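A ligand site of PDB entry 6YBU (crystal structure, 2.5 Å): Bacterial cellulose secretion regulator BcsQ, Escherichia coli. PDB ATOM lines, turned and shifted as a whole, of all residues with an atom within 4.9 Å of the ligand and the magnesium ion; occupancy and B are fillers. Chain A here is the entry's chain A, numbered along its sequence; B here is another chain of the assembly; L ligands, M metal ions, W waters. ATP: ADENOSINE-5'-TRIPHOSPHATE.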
ATOM      1  N   ARG A  10     -12.304  -4.658 -22.095  1.00  0.00           N
ATOM      2  CA  ARG A  10     -12.326  -6.050 -22.516  1.00  0.00           C
ATOM      3  C   ARG A  10     -10.891  -6.564 -22.445  1.00  0.00           C
ATOM      4  O   ARG A  10      -9.939  -5.790 -22.498  1.00  0.00           O
ATOM      5  CB  ARG A  10     -12.926  -6.177 -23.923  1.00  0.00           C
ATOM      6  CG  ARG A  10     -13.015  -7.578 -24.474  1.00  0.00           C
ATOM      7  CD  ARG A  10     -12.191  -7.704 -25.744  1.00  0.00           C
ATOM      8  NE  ARG A  10     -12.577  -6.749 -26.777  1.00  0.00           N
ATOM      9  CZ  ARG A  10     -11.896  -6.550 -27.901  1.00  0.00           C
ATOM     10  NH1 ARG A  10     -10.787  -7.238 -28.146  1.00  0.00           N
ATOM     11  NH2 ARG A  10     -12.320  -5.661 -28.788  1.00  0.00           N
ATOM     12  N   GLY A  11     -10.758  -7.879 -22.295  1.00  0.00           N
ATOM     13  CA  GLY A  11      -9.424  -8.458 -22.285  1.00  0.00           C
ATOM     14  C   GLY A  11      -8.742  -8.317 -23.628  1.00  0.00           C
ATOM     15  O   GLY A  11      -9.364  -8.369 -24.692  1.00  0.00           O
ATOM     16  N   GLY A  12      -7.426  -8.113 -23.579  1.00  0.00           N
ATOM     17  CA  GLY A  12      -6.628  -8.092 -24.787  1.00  0.00           C
ATOM     18  C   GLY A  12      -6.800  -6.884 -25.685  1.00  0.00           C
ATOM     19  O   GLY A  12      -6.698  -7.011 -26.906  1.00  0.00           O
ATOM     20  N   VAL A  13      -7.065  -5.707 -25.107  1.00  0.00           N
ATOM     21  CA  VAL A  13      -7.176  -4.478 -25.884  1.00  0.00           C
ATOM     22  C   VAL A  13      -5.900  -3.649 -25.850  1.00  0.00           C
ATOM     23  O   VAL A  13      -5.840  -2.598 -26.510  1.00  0.00           O
ATOM     24  CB  VAL A  13      -8.380  -3.633 -25.421  1.00  0.00           C
ATOM     25  CG1 VAL A  13      -9.680  -4.365 -25.725  1.00  0.00           C
ATOM     26  CG2 VAL A  13      -8.265  -3.327 -23.937  1.00  0.00           C
ATOM     27  N   GLY A  14      -4.896  -4.078 -25.100  1.00  0.00           N
ATOM     28  CA  GLY A  14      -3.631  -3.380 -25.012  1.00  0.00           C
ATOM     29  C   GLY A  14      -3.327  -2.709 -23.682  1.00  0.00           C
ATOM     30  O   GLY A  14      -2.406  -1.871 -23.635  1.00  0.00           O
ATOM     31  N   THR A  15      -4.040  -3.056 -22.614  1.00  0.00           N
ATOM     32  CA  THR A  15      -3.915  -2.312 -21.359  1.00  0.00           C
ATOM     33  C   THR A  15      -2.510  -2.398 -20.781  1.00  0.00           C
ATOM     34  O   THR A  15      -1.926  -1.386 -20.375  1.00  0.00           O
ATOM     35  CB  THR A  15      -4.941  -2.845 -20.347  1.00  0.00           C
ATOM     36  OG1 THR A  15      -6.259  -2.742 -20.898  1.00  0.00           O
ATOM     37  CG2 THR A  15      -4.870  -2.048 -19.054  1.00  0.00           C
ATOM     38  N   THR A  16      -1.938  -3.606 -20.749  1.00  0.00           N
ATOM     39  CA  THR A  16      -0.624  -3.783 -20.119  1.00  0.00           C
ATOM     40  C   THR A  16       0.469  -3.083 -20.923  1.00  0.00           C
ATOM     41  O   THR A  16       1.313  -2.380 -20.365  1.00  0.00           O
ATOM     42  CB  THR A  16      -0.313  -5.265 -19.973  1.00  0.00           C
ATOM     43  OG1 THR A  16      -1.382  -5.905 -19.265  1.00  0.00           O
ATOM     44  CG2 THR A  16       0.974  -5.463 -19.201  1.00  0.00           C
ATOM     45  N   THR A  17       0.473  -3.282 -22.254  1.00  0.00           N
ATOM     46  CA  THR A  17       1.474  -2.629 -23.096  1.00  0.00           C
ATOM     47  C   THR A  17       1.388  -1.114 -22.979  1.00  0.00           C
ATOM     48  O   THR A  17       2.412  -0.438 -22.925  1.00  0.00           O
ATOM     49  CB  THR A  17       1.290  -3.071 -24.545  1.00  0.00           C
ATOM     50  OG1 THR A  17       1.434  -4.496 -24.649  1.00  0.00           O
ATOM     51  CG2 THR A  17       2.323  -2.408 -25.450  1.00  0.00           C
ATOM     52  N   ILE A  18       0.172  -0.572 -22.930  1.00  0.00           N
ATOM     53  CA  ILE A  18       0.010   0.873 -22.793  1.00  0.00           C
ATOM     54  C   ILE A  18       0.495   1.347 -21.429  1.00  0.00           C
ATOM     55  O   ILE A  18       1.125   2.399 -21.313  1.00  0.00           O
ATOM     56  CB  ILE A  18      -1.455   1.275 -23.058  1.00  0.00           C
ATOM     57  CG1 ILE A  18      -1.832   1.012 -24.518  1.00  0.00           C
ATOM     58  CG2 ILE A  18      -1.680   2.739 -22.712  1.00  0.00           C
ATOM     59  CD1 ILE A  18      -3.306   1.223 -24.818  1.00  0.00           C
ATOM     60  N   CYS A  39      -3.022  -7.024 -12.072  1.00  0.00           N
ATOM     61  CA  CYS A  39      -3.624  -8.148 -12.784  1.00  0.00           C
ATOM     62  C   CYS A  39      -2.940  -9.441 -12.350  1.00  0.00           C
ATOM     63  O   CYS A  39      -1.713  -9.533 -12.390  1.00  0.00           O
ATOM     64  CB  CYS A  39      -3.488  -7.975 -14.293  1.00  0.00           C
ATOM     65  SG  CYS A  39      -4.327  -9.243 -15.254  1.00  0.00           S
ATOM     66  N   LEU A  43       1.800 -10.054 -16.046  1.00  0.00           N
ATOM     67  CA  LEU A  43       2.406  -9.873 -17.353  1.00  0.00           C
ATOM     68  C   LEU A  43       3.138  -8.546 -17.501  1.00  0.00           C
ATOM     69  O   LEU A  43       3.983  -8.421 -18.393  1.00  0.00           O
ATOM     70  CB  LEU A  43       1.344  -9.970 -18.454  1.00  0.00           C
ATOM     71  CG  LEU A  43       0.642 -11.325 -18.582  1.00  0.00           C
ATOM     72  CD1 LEU A  43      -0.502 -11.243 -19.580  1.00  0.00           C
ATOM     73  CD2 LEU A  43       1.641 -12.386 -18.999  1.00  0.00           C
ATOM     74  N   ASP A 124      -1.961  -1.200 -13.475  1.00  0.00           N
ATOM     75  CA  ASP A 124      -2.495  -2.059 -14.517  1.00  0.00           C
ATOM     76  C   ASP A 124      -3.609  -2.902 -13.901  1.00  0.00           C
ATOM     77  O   ASP A 124      -3.340  -3.868 -13.188  1.00  0.00           O
ATOM     78  CB  ASP A 124      -1.392  -2.930 -15.109  1.00  0.00           C
ATOM     79  CG  ASP A 124      -1.864  -3.816 -16.247  1.00  0.00           C
ATOM     80  OD1 ASP A 124      -3.040  -3.692 -16.662  1.00  0.00           O
ATOM     81  OD2 ASP A 124      -1.062  -4.645 -16.718  1.00  0.00           O
ATOM     82  N   ASN A 171      -7.096   2.032 -28.849  1.00  0.00           N
ATOM     83  CA  ASN A 171      -5.859   1.350 -29.193  1.00  0.00           C
ATOM     84  C   ASN A 171      -6.089   0.463 -30.409  1.00  0.00           C
ATOM     85  O   ASN A 171      -7.218   0.076 -30.720  1.00  0.00           O
ATOM     86  CB  ASN A 171      -5.338   0.517 -28.016  1.00  0.00           C
ATOM     87  CG  ASN A 171      -3.966  -0.084 -28.299  1.00  0.00           C
ATOM     88  OD1 ASN A 171      -3.090   0.573 -28.875  1.00  0.00           O
ATOM     89  ND2 ASN A 171      -3.773  -1.338 -27.899  1.00  0.00           N
ATOM     90  N   ASN A 172      -4.981   0.152 -31.098  1.00  0.00           N
ATOM     91  CA  ASN A 172      -4.968  -0.793 -32.213  1.00  0.00           C
ATOM     92  C   ASN A 172      -5.800  -0.296 -33.392  1.00  0.00           C
ATOM     93  O   ASN A 172      -6.341  -1.101 -34.162  1.00  0.00           O
ATOM     94  CB  ASN A 172      -5.419  -2.189 -31.773  1.00  0.00           C
ATOM     95  CG  ASN A 172      -4.677  -3.297 -32.499  1.00  0.00           C
ATOM     96  OD1 ASN A 172      -5.080  -3.740 -33.566  1.00  0.00           O
ATOM     97  ND2 ASN A 172      -3.580  -3.743 -31.907  1.00  0.00           N
ATOM     98  N   ILE A 199      -4.156   5.460 -30.422  1.00  0.00           N
ATOM     99  CA  ILE A 199      -2.965   4.672 -30.709  1.00  0.00           C
ATOM    100  C   ILE A 199      -3.294   3.740 -31.861  1.00  0.00           C
ATOM    101  O   ILE A 199      -4.244   2.945 -31.767  1.00  0.00           O
ATOM    102  CB  ILE A 199      -2.498   3.878 -29.475  1.00  0.00           C
ATOM    103  CG1 ILE A 199      -2.415   4.803 -28.261  1.00  0.00           C
ATOM    104  CG2 ILE A 199      -1.150   3.229 -29.751  1.00  0.00           C
ATOM    105  CD1 ILE A 199      -2.364   4.072 -26.943  1.00  0.00           C
ATOM    106  N   HIS A 200      -2.519   3.829 -32.941  1.00  0.00           N
ATOM    107  CA  HIS A 200      -2.728   2.970 -34.090  1.00  0.00           C
ATOM    108  C   HIS A 200      -2.172   1.576 -33.837  1.00  0.00           C
ATOM    109  O   HIS A 200      -1.351   1.350 -32.944  1.00  0.00           O
ATOM    110  CB  HIS A 200      -2.050   3.554 -35.327  1.00  0.00           C
ATOM    111  CG  HIS A 200      -2.806   4.660 -35.978  1.00  0.00           C
ATOM    112  ND1 HIS A 200      -2.727   5.978 -35.554  1.00  0.00           N
ATOM    113  CD2 HIS A 200      -3.654   4.664 -37.043  1.00  0.00           C
ATOM    114  CE1 HIS A 200      -3.491   6.735 -36.317  1.00  0.00           C
ATOM    115  NE2 HIS A 200      -4.062   5.972 -37.228  1.00  0.00           N
ATOM    116  N   ARG A 201      -2.660   0.619 -34.633  1.00  0.00           N
ATOM    117  CA  ARG A 201      -1.966  -0.644 -34.792  1.00  0.00           C
ATOM    118  C   ARG A 201      -0.537  -0.383 -35.253  1.00  0.00           C
ATOM    119  O   ARG A 201      -0.312   0.428 -36.171  1.00  0.00           O
ATOM    120  CB  ARG A 201      -2.709  -1.528 -35.796  1.00  0.00           C
ATOM    121  CG  ARG A 201      -1.941  -2.753 -36.256  1.00  0.00           C
ATOM    122  CD  ARG A 201      -2.190  -3.958 -35.369  1.00  0.00           C
ATOM    123  NE  ARG A 201      -1.266  -5.053 -35.661  1.00  0.00           N
ATOM    124  CZ  ARG A 201      -1.145  -6.147 -34.913  1.00  0.00           C
ATOM    125  NH1 ARG A 201      -1.887  -6.295 -33.826  1.00  0.00           N
ATOM    126  NH2 ARG A 201      -0.269  -7.081 -35.255  1.00  0.00           N
ATOM    127  N   ASP A 202       0.422  -1.042 -34.616  1.00  0.00           N
ATOM    128  CA  ASP A 202       1.830  -0.746 -34.864  1.00  0.00           C
ATOM    129  C   ASP A 202       2.651  -1.990 -34.568  1.00  0.00           C
ATOM    130  O   ASP A 202       2.571  -2.528 -33.472  1.00  0.00           O
ATOM    131  CB  ASP A 202       2.294   0.429 -33.994  1.00  0.00           C
ATOM    132  CG  ASP A 202       3.612   1.029 -34.463  1.00  0.00           C
ATOM    133  OD1 ASP A 202       4.488   0.274 -34.929  1.00  0.00           O
ATOM    134  OD2 ASP A 202       3.776   2.264 -34.352  1.00  0.00           O
ATOM    135  N   MET A 205       4.453  -2.090 -31.365  1.00  0.00           N
ATOM    136  CA  MET A 205       3.707  -2.477 -30.163  1.00  0.00           C
ATOM    137  C   MET A 205       3.613  -3.987 -30.017  1.00  0.00           C
ATOM    138  O   MET A 205       3.534  -4.499 -28.901  1.00  0.00           O
ATOM    139  CB  MET A 205       2.309  -1.860 -30.203  1.00  0.00           C
ATOM    140  CG  MET A 205       2.287  -0.368 -29.992  1.00  0.00           C
ATOM    141  SD  MET A 205       2.472   0.106 -28.262  1.00  0.00           S
ATOM    142  CE  MET A 205       0.790  -0.039 -27.689  1.00  0.00           C
ATOM    143  N   ALA A 206       3.608  -4.714 -31.136  1.00  0.00           N
ATOM    144  CA  ALA A 206       3.618  -6.176 -31.063  1.00  0.00           C
ATOM    145  C   ALA A 206       5.007  -6.719 -30.791  1.00  0.00           C
ATOM    146  O   ALA A 206       5.144  -7.800 -30.207  1.00  0.00           O
ATOM    147  CB  ALA A 206       3.066  -6.776 -32.352  1.00  0.00           C
ATOM    148  N   LEU A 209       6.970  -6.360 -26.706  1.00  0.00           N
ATOM    149  CA  LEU A 209       6.777  -7.381 -25.681  1.00  0.00           C
ATOM    150  C   LEU A 209       7.680  -8.577 -25.924  1.00  0.00           C
ATOM    151  O   LEU A 209       8.171  -9.200 -24.970  1.00  0.00           O
ATOM    152  CB  LEU A 209       5.304  -7.807 -25.627  1.00  0.00           C
ATOM    153  CG  LEU A 209       4.931  -8.814 -24.535  1.00  0.00           C
ATOM    154  CD1 LEU A 209       5.534  -8.417 -23.197  1.00  0.00           C
ATOM    155  CD2 LEU A 209       3.418  -8.946 -24.423  1.00  0.00           C
ATOM    156  N   ARG B  10      -7.335 -15.873 -23.439  1.00  0.00           N
ATOM    157  CA  ARG B  10      -7.296 -14.462 -23.120  1.00  0.00           C
ATOM    158  C   ARG B  10      -8.599 -13.853 -23.630  1.00  0.00           C
ATOM    159  O   ARG B  10      -9.324 -14.479 -24.406  1.00  0.00           O
ATOM    160  CB  ARG B  10      -6.071 -13.791 -23.763  1.00  0.00           C
ATOM    161  CG  ARG B  10      -5.783 -12.370 -23.316  1.00  0.00           C
ATOM    162  CD  ARG B  10      -5.730 -11.441 -24.524  1.00  0.00           C
ATOM    163  NE  ARG B  10      -4.673 -11.790 -25.463  1.00  0.00           N
ATOM    164  CZ  ARG B  10      -4.687 -11.479 -26.754  1.00  0.00           C
ATOM    165  NH1 ARG B  10      -5.714 -10.813 -27.259  1.00  0.00           N
ATOM    166  NH2 ARG B  10      -3.678 -11.837 -27.532  1.00  0.00           N
ATOM    167  N   GLY B  11      -8.901 -12.650 -23.178  1.00  0.00           N
ATOM    168  CA  GLY B  11     -10.053 -11.943 -23.684  1.00  0.00           C
ATOM    169  C   GLY B  11      -9.791 -11.370 -25.075  1.00  0.00           C
ATOM    170  O   GLY B  11      -8.664 -11.078 -25.453  1.00  0.00           O
ATOM    171  N   ASP B 150       0.521 -13.733 -30.840  1.00  0.00           N
ATOM    172  CA  ASP B 150       1.253 -12.596 -30.294  1.00  0.00           C
ATOM    173  C   ASP B 150       1.989 -13.045 -29.040  1.00  0.00           C
ATOM    174  O   ASP B 150       1.828 -14.168 -28.573  1.00  0.00           O
ATOM    175  CB  ASP B 150       0.318 -11.406 -30.010  1.00  0.00           C
ATOM    176  CG  ASP B 150      -0.873 -11.793 -29.147  1.00  0.00           C
ATOM    177  OD1 ASP B 150      -0.653 -12.335 -28.043  1.00  0.00           O
ATOM    178  OD2 ASP B 150      -2.018 -11.526 -29.567  1.00  0.00           O
ATOM    179  N   ALA B 151       2.808 -12.129 -28.515  1.00  0.00           N
ATOM    180  CA  ALA B 151       3.645 -12.462 -27.359  1.00  0.00           C
ATOM    181  C   ALA B 151       2.803 -12.720 -26.113  1.00  0.00           C
ATOM    182  O   ALA B 151       3.212 -13.513 -25.247  1.00  0.00           O
ATOM    183  CB  ALA B 151       4.636 -11.342 -27.098  1.00  0.00           C
ATOM    184  N   ASN B 152       1.645 -12.073 -25.988  1.00  0.00           N
ATOM    185  CA  ASN B 152       0.779 -12.281 -24.831  1.00  0.00           C
ATOM    186  C   ASN B 152       0.344 -13.740 -24.744  1.00  0.00           C
ATOM    187  O   ASN B 152       0.542 -14.411 -23.719  1.00  0.00           O
ATOM    188  CB  ASN B 152      -0.430 -11.347 -24.913  1.00  0.00           C
ATOM    189  CG  ASN B 152      -1.365 -11.473 -23.715  1.00  0.00           C
ATOM    190  OD1 ASN B 152      -1.874 -12.552 -23.406  1.00  0.00           O
ATOM    191  ND2 ASN B 152      -1.599 -10.359 -23.038  1.00  0.00           N
ATOM    192  N   ARG B 156       1.146 -16.905 -22.138  1.00  0.00           N
ATOM    193  CA  ARG B 156       0.060 -17.594 -21.456  1.00  0.00           C
ATOM    194  C   ARG B 156       0.130 -19.106 -21.673  1.00  0.00           C
ATOM    195  O   ARG B 156      -0.182 -19.878 -20.762  1.00  0.00           O
ATOM    196  CB  ARG B 156      -1.292 -17.054 -21.932  1.00  0.00           C
ATOM    197  CG  ARG B 156      -1.550 -15.614 -21.517  1.00  0.00           C
ATOM    198  CD  ARG B 156      -2.952 -15.194 -21.931  1.00  0.00           C
ATOM    199  NE  ARG B 156      -3.307 -13.867 -21.428  1.00  0.00           N
ATOM    200  CZ  ARG B 156      -3.802 -13.638 -20.216  1.00  0.00           C
ATOM    201  NH1 ARG B 156      -4.011 -14.644 -19.381  1.00  0.00           N
ATOM    202  NH2 ARG B 156      -4.098 -12.403 -19.844  1.00  0.00           N
HETATM  203  PG  ATP L   1      -4.835  -9.044 -21.169  1.00  0.00           P
HETATM  204  O1G ATP L   1      -6.312  -9.153 -21.371  1.00  0.00           O
HETATM  205  O2G ATP L   1      -4.465  -8.416 -19.833  1.00  0.00           O
HETATM  206  O3G ATP L   1      -4.110 -10.385 -21.294  1.00  0.00           O
HETATM  207  PB  ATP L   1      -4.155  -6.501 -22.409  1.00  0.00           P
HETATM  208  O1B ATP L   1      -5.502  -5.907 -22.525  1.00  0.00           O
HETATM  209  O2B ATP L   1      -3.295  -5.982 -21.252  1.00  0.00           O
HETATM  210  O3B ATP L   1      -4.204  -8.083 -22.277  1.00  0.00           O
HETATM  211  PA  ATP L   1      -1.747  -6.385 -24.045  1.00  0.00           P
HETATM  212  O1A ATP L   1      -1.093  -7.490 -23.305  1.00  0.00           O
HETATM  213  O2A ATP L   1      -1.180  -5.002 -23.788  1.00  0.00           O
HETATM  214  O3A ATP L   1      -3.312  -6.316 -23.737  1.00  0.00           O
HETATM  215  O5' ATP L   1      -1.724  -6.631 -25.627  1.00  0.00           O
HETATM  216  C5' ATP L   1      -2.011  -7.932 -26.173  1.00  0.00           C
HETATM  217  C4' ATP L   1      -1.093  -8.207 -27.330  1.00  0.00           C
HETATM  218  O4' ATP L   1      -1.351  -7.254 -28.392  1.00  0.00           O
HETATM  219  C3' ATP L   1       0.401  -8.101 -27.028  1.00  0.00           C
HETATM  220  O3' ATP L   1       1.136  -9.086 -27.749  1.00  0.00           O
HETATM  221  C2' ATP L   1       0.748  -6.676 -27.486  1.00  0.00           C
HETATM  222  O2' ATP L   1       2.109  -6.567 -27.892  1.00  0.00           O
HETATM  223  C1' ATP L   1      -0.182  -6.515 -28.689  1.00  0.00           C
HETATM  224  N9  ATP L   1      -0.571  -5.140 -28.958  1.00  0.00           N
HETATM  225  C8  ATP L   1      -1.145  -4.250 -28.084  1.00  0.00           C
HETATM  226  N7  ATP L   1      -1.382  -3.071 -28.590  1.00  0.00           N
HETATM  227  C5  ATP L   1      -0.939  -3.188 -29.907  1.00  0.00           C
HETATM  228  C6  ATP L   1      -0.908  -2.276 -30.980  1.00  0.00           C
HETATM  229  N6  ATP L   1      -1.338  -1.010 -30.898  1.00  0.00           N
HETATM  230  N1  ATP L   1      -0.393  -2.712 -32.149  1.00  0.00           N
HETATM  231  C2  ATP L   1       0.048  -3.965 -32.232  1.00  0.00           C
HETATM  232  N3  ATP L   1       0.076  -4.906 -31.292  1.00  0.00           N
HETATM  233  C4  ATP L   1      -0.441  -4.455 -30.143  1.00  0.00           C
HETATM  234 MG    MG M   1      -3.065  -7.159 -19.262  1.00  0.00          MG
HETATM  235  O   HOH W   1      -1.626  -8.231 -20.517  1.00  0.00           O
HETATM  236  O   HOH W   2      -2.451  -8.240 -17.633  1.00  0.00           O
HETATM  237  O   HOH W   3      -7.853 -11.376 -20.848  1.00  0.00           O
HETATM  238  O   HOH W   4      -4.246  -5.543 -18.487  1.00  0.00           O
HETATM  239  O   HOH W   5      -7.609  -5.410 -20.995  1.00  0.00           O
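The backbone NH (N) of Thr 16 sits at hydrogen-bond distance from an oxygen (O2A) of the ligand.
An oxygen (O3G) of the ligand is in salt-bridge range of the guanidinium group of Arg 156 of chain B, at 2.5 Å.
An oxygen (O1G) of the ligand is in hydrogen-bond range of the backbone NH (N) of Gly 12 (2.7 Å).
O of Met 205 sits at hydrogen-bond distance from O2' of the ligand, at 2.7 Å.
N of Thr 17 lies within hydrogen-bond range of O2A of the ligand (2.8 Å).
An oxygen (O2A) of the ligand is in hydrogen-bond range of the side-chain hydroxyl (OG1) of Thr 17, at 2.8 Å.
O1A of the ligand is in hydrogen-bond range of ND2 of Asn 152 of chain B (2.9 Å).
N of Val 13 sits at hydrogen-bond distance from O1B of the ligand (3.0 Å).
ND2 of Asn 171 sits at hydrogen-bond distance from N7 of the ligand (3.0 Å).
The backbone NH (N) of Gly 14 lies within hydrogen-bond range of an oxygen (O3A) of the ligand (3.1 Å).
The backbone NH (N) of Asp 202 sits at hydrogen-bond distance from a nitrogen (N1) of the ligand, at 3.1 Å.
The backbone carbonyl oxygen of His 200 sits at hydrogen-bond distance from a nitrogen (N6) of the ligand (3.1 Å).
ND2 of Asn 172 sits close to N1 of the ligand.
The backbone NH (N) of Thr 15 lies within hydrogen-bond range of an oxygen (O1B) of the ligand (3.2 Å).
A nitrogen (N3) of the ligand sits close to the guanidinium group of Arg 201.
OG1 of Thr 16 lies close to OD2 of Asp 124, at 2.9 Å.
The guanidinium group (NE) of Arg 156 of chain B is in hydrogen-bond range of the side-chain amide oxygen (OD1) of Asn 152 of chain B, at 2.8 Å.
OD1 of Asp 150 of chain B is in hydrogen-bond range of N of Asn 152 of chain B (3.1 Å).
O of Val 13 sits at hydrogen-bond distance from ND2 of Asn 171, at 2.8 Å.
The backbone NH (N) of Asn 172 is in hydrogen-bond range of the backbone carbonyl oxygen (O) of Ile 199, at 3.0 Å.
The guanidinium group of Arg 10 of chain B is in salt-bridge range of the side-chain carboxylate of Asp 150 of chain B, at 2.6 Å.
Gly 11 of chain A touches the ligand (CA to O1G, 3.3 Å).
Ala 206 touches the ligand (CA to O2', 3.5 Å).
CG of Arg 10 of chain B touches O3G of the ligand, 3.3 Å away.
Asp 150 of chain B touches the ligand (CB to O3', 3.3 Å).
Ala 151 of chain B touches the ligand.
Hydrophobic or aromatic side chains within 4 Å of the ligand: Met 205 and Ala 206.
The nearest printed residue that does not touch the ligand is Leu 209 (4.04 Å).
One residue has an atom within 4 Å of the magnesium ion: Thr 16.
The nearest printed residue that does not touch the magnesium ion is Asp 124 (4.1 Å).
The magnesium ion is bound by an oxygen (O2G) of the ligand (2.0 Å), water W2 (2.0 Å), the side-chain hydroxyl (OG1) of Thr 16 (2.1 Å), water W4 (2.1 Å), water W1 (2.2 Å) and an oxygen (O2B) of the ligand (2.3 Å).
The magnesium ion has six donor atoms within binding distance.
Water W1 bridges O1A of the ligand and ND2 of Asn 152 of chain B.
Water W5 lies within hydrogen-bond range of an oxygen (O1B) of the ligand (2.7 Å), the backbone carbonyl oxygen of Arg 10 of chain A (2.8 Å) and the side-chain hydroxyl of Thr 15 (3.0 Å).
Water W3 lies within hydrogen-bond range of O1G of the ligand (2.8 Å) and N of Gly 11 of chain B (2.9 Å).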
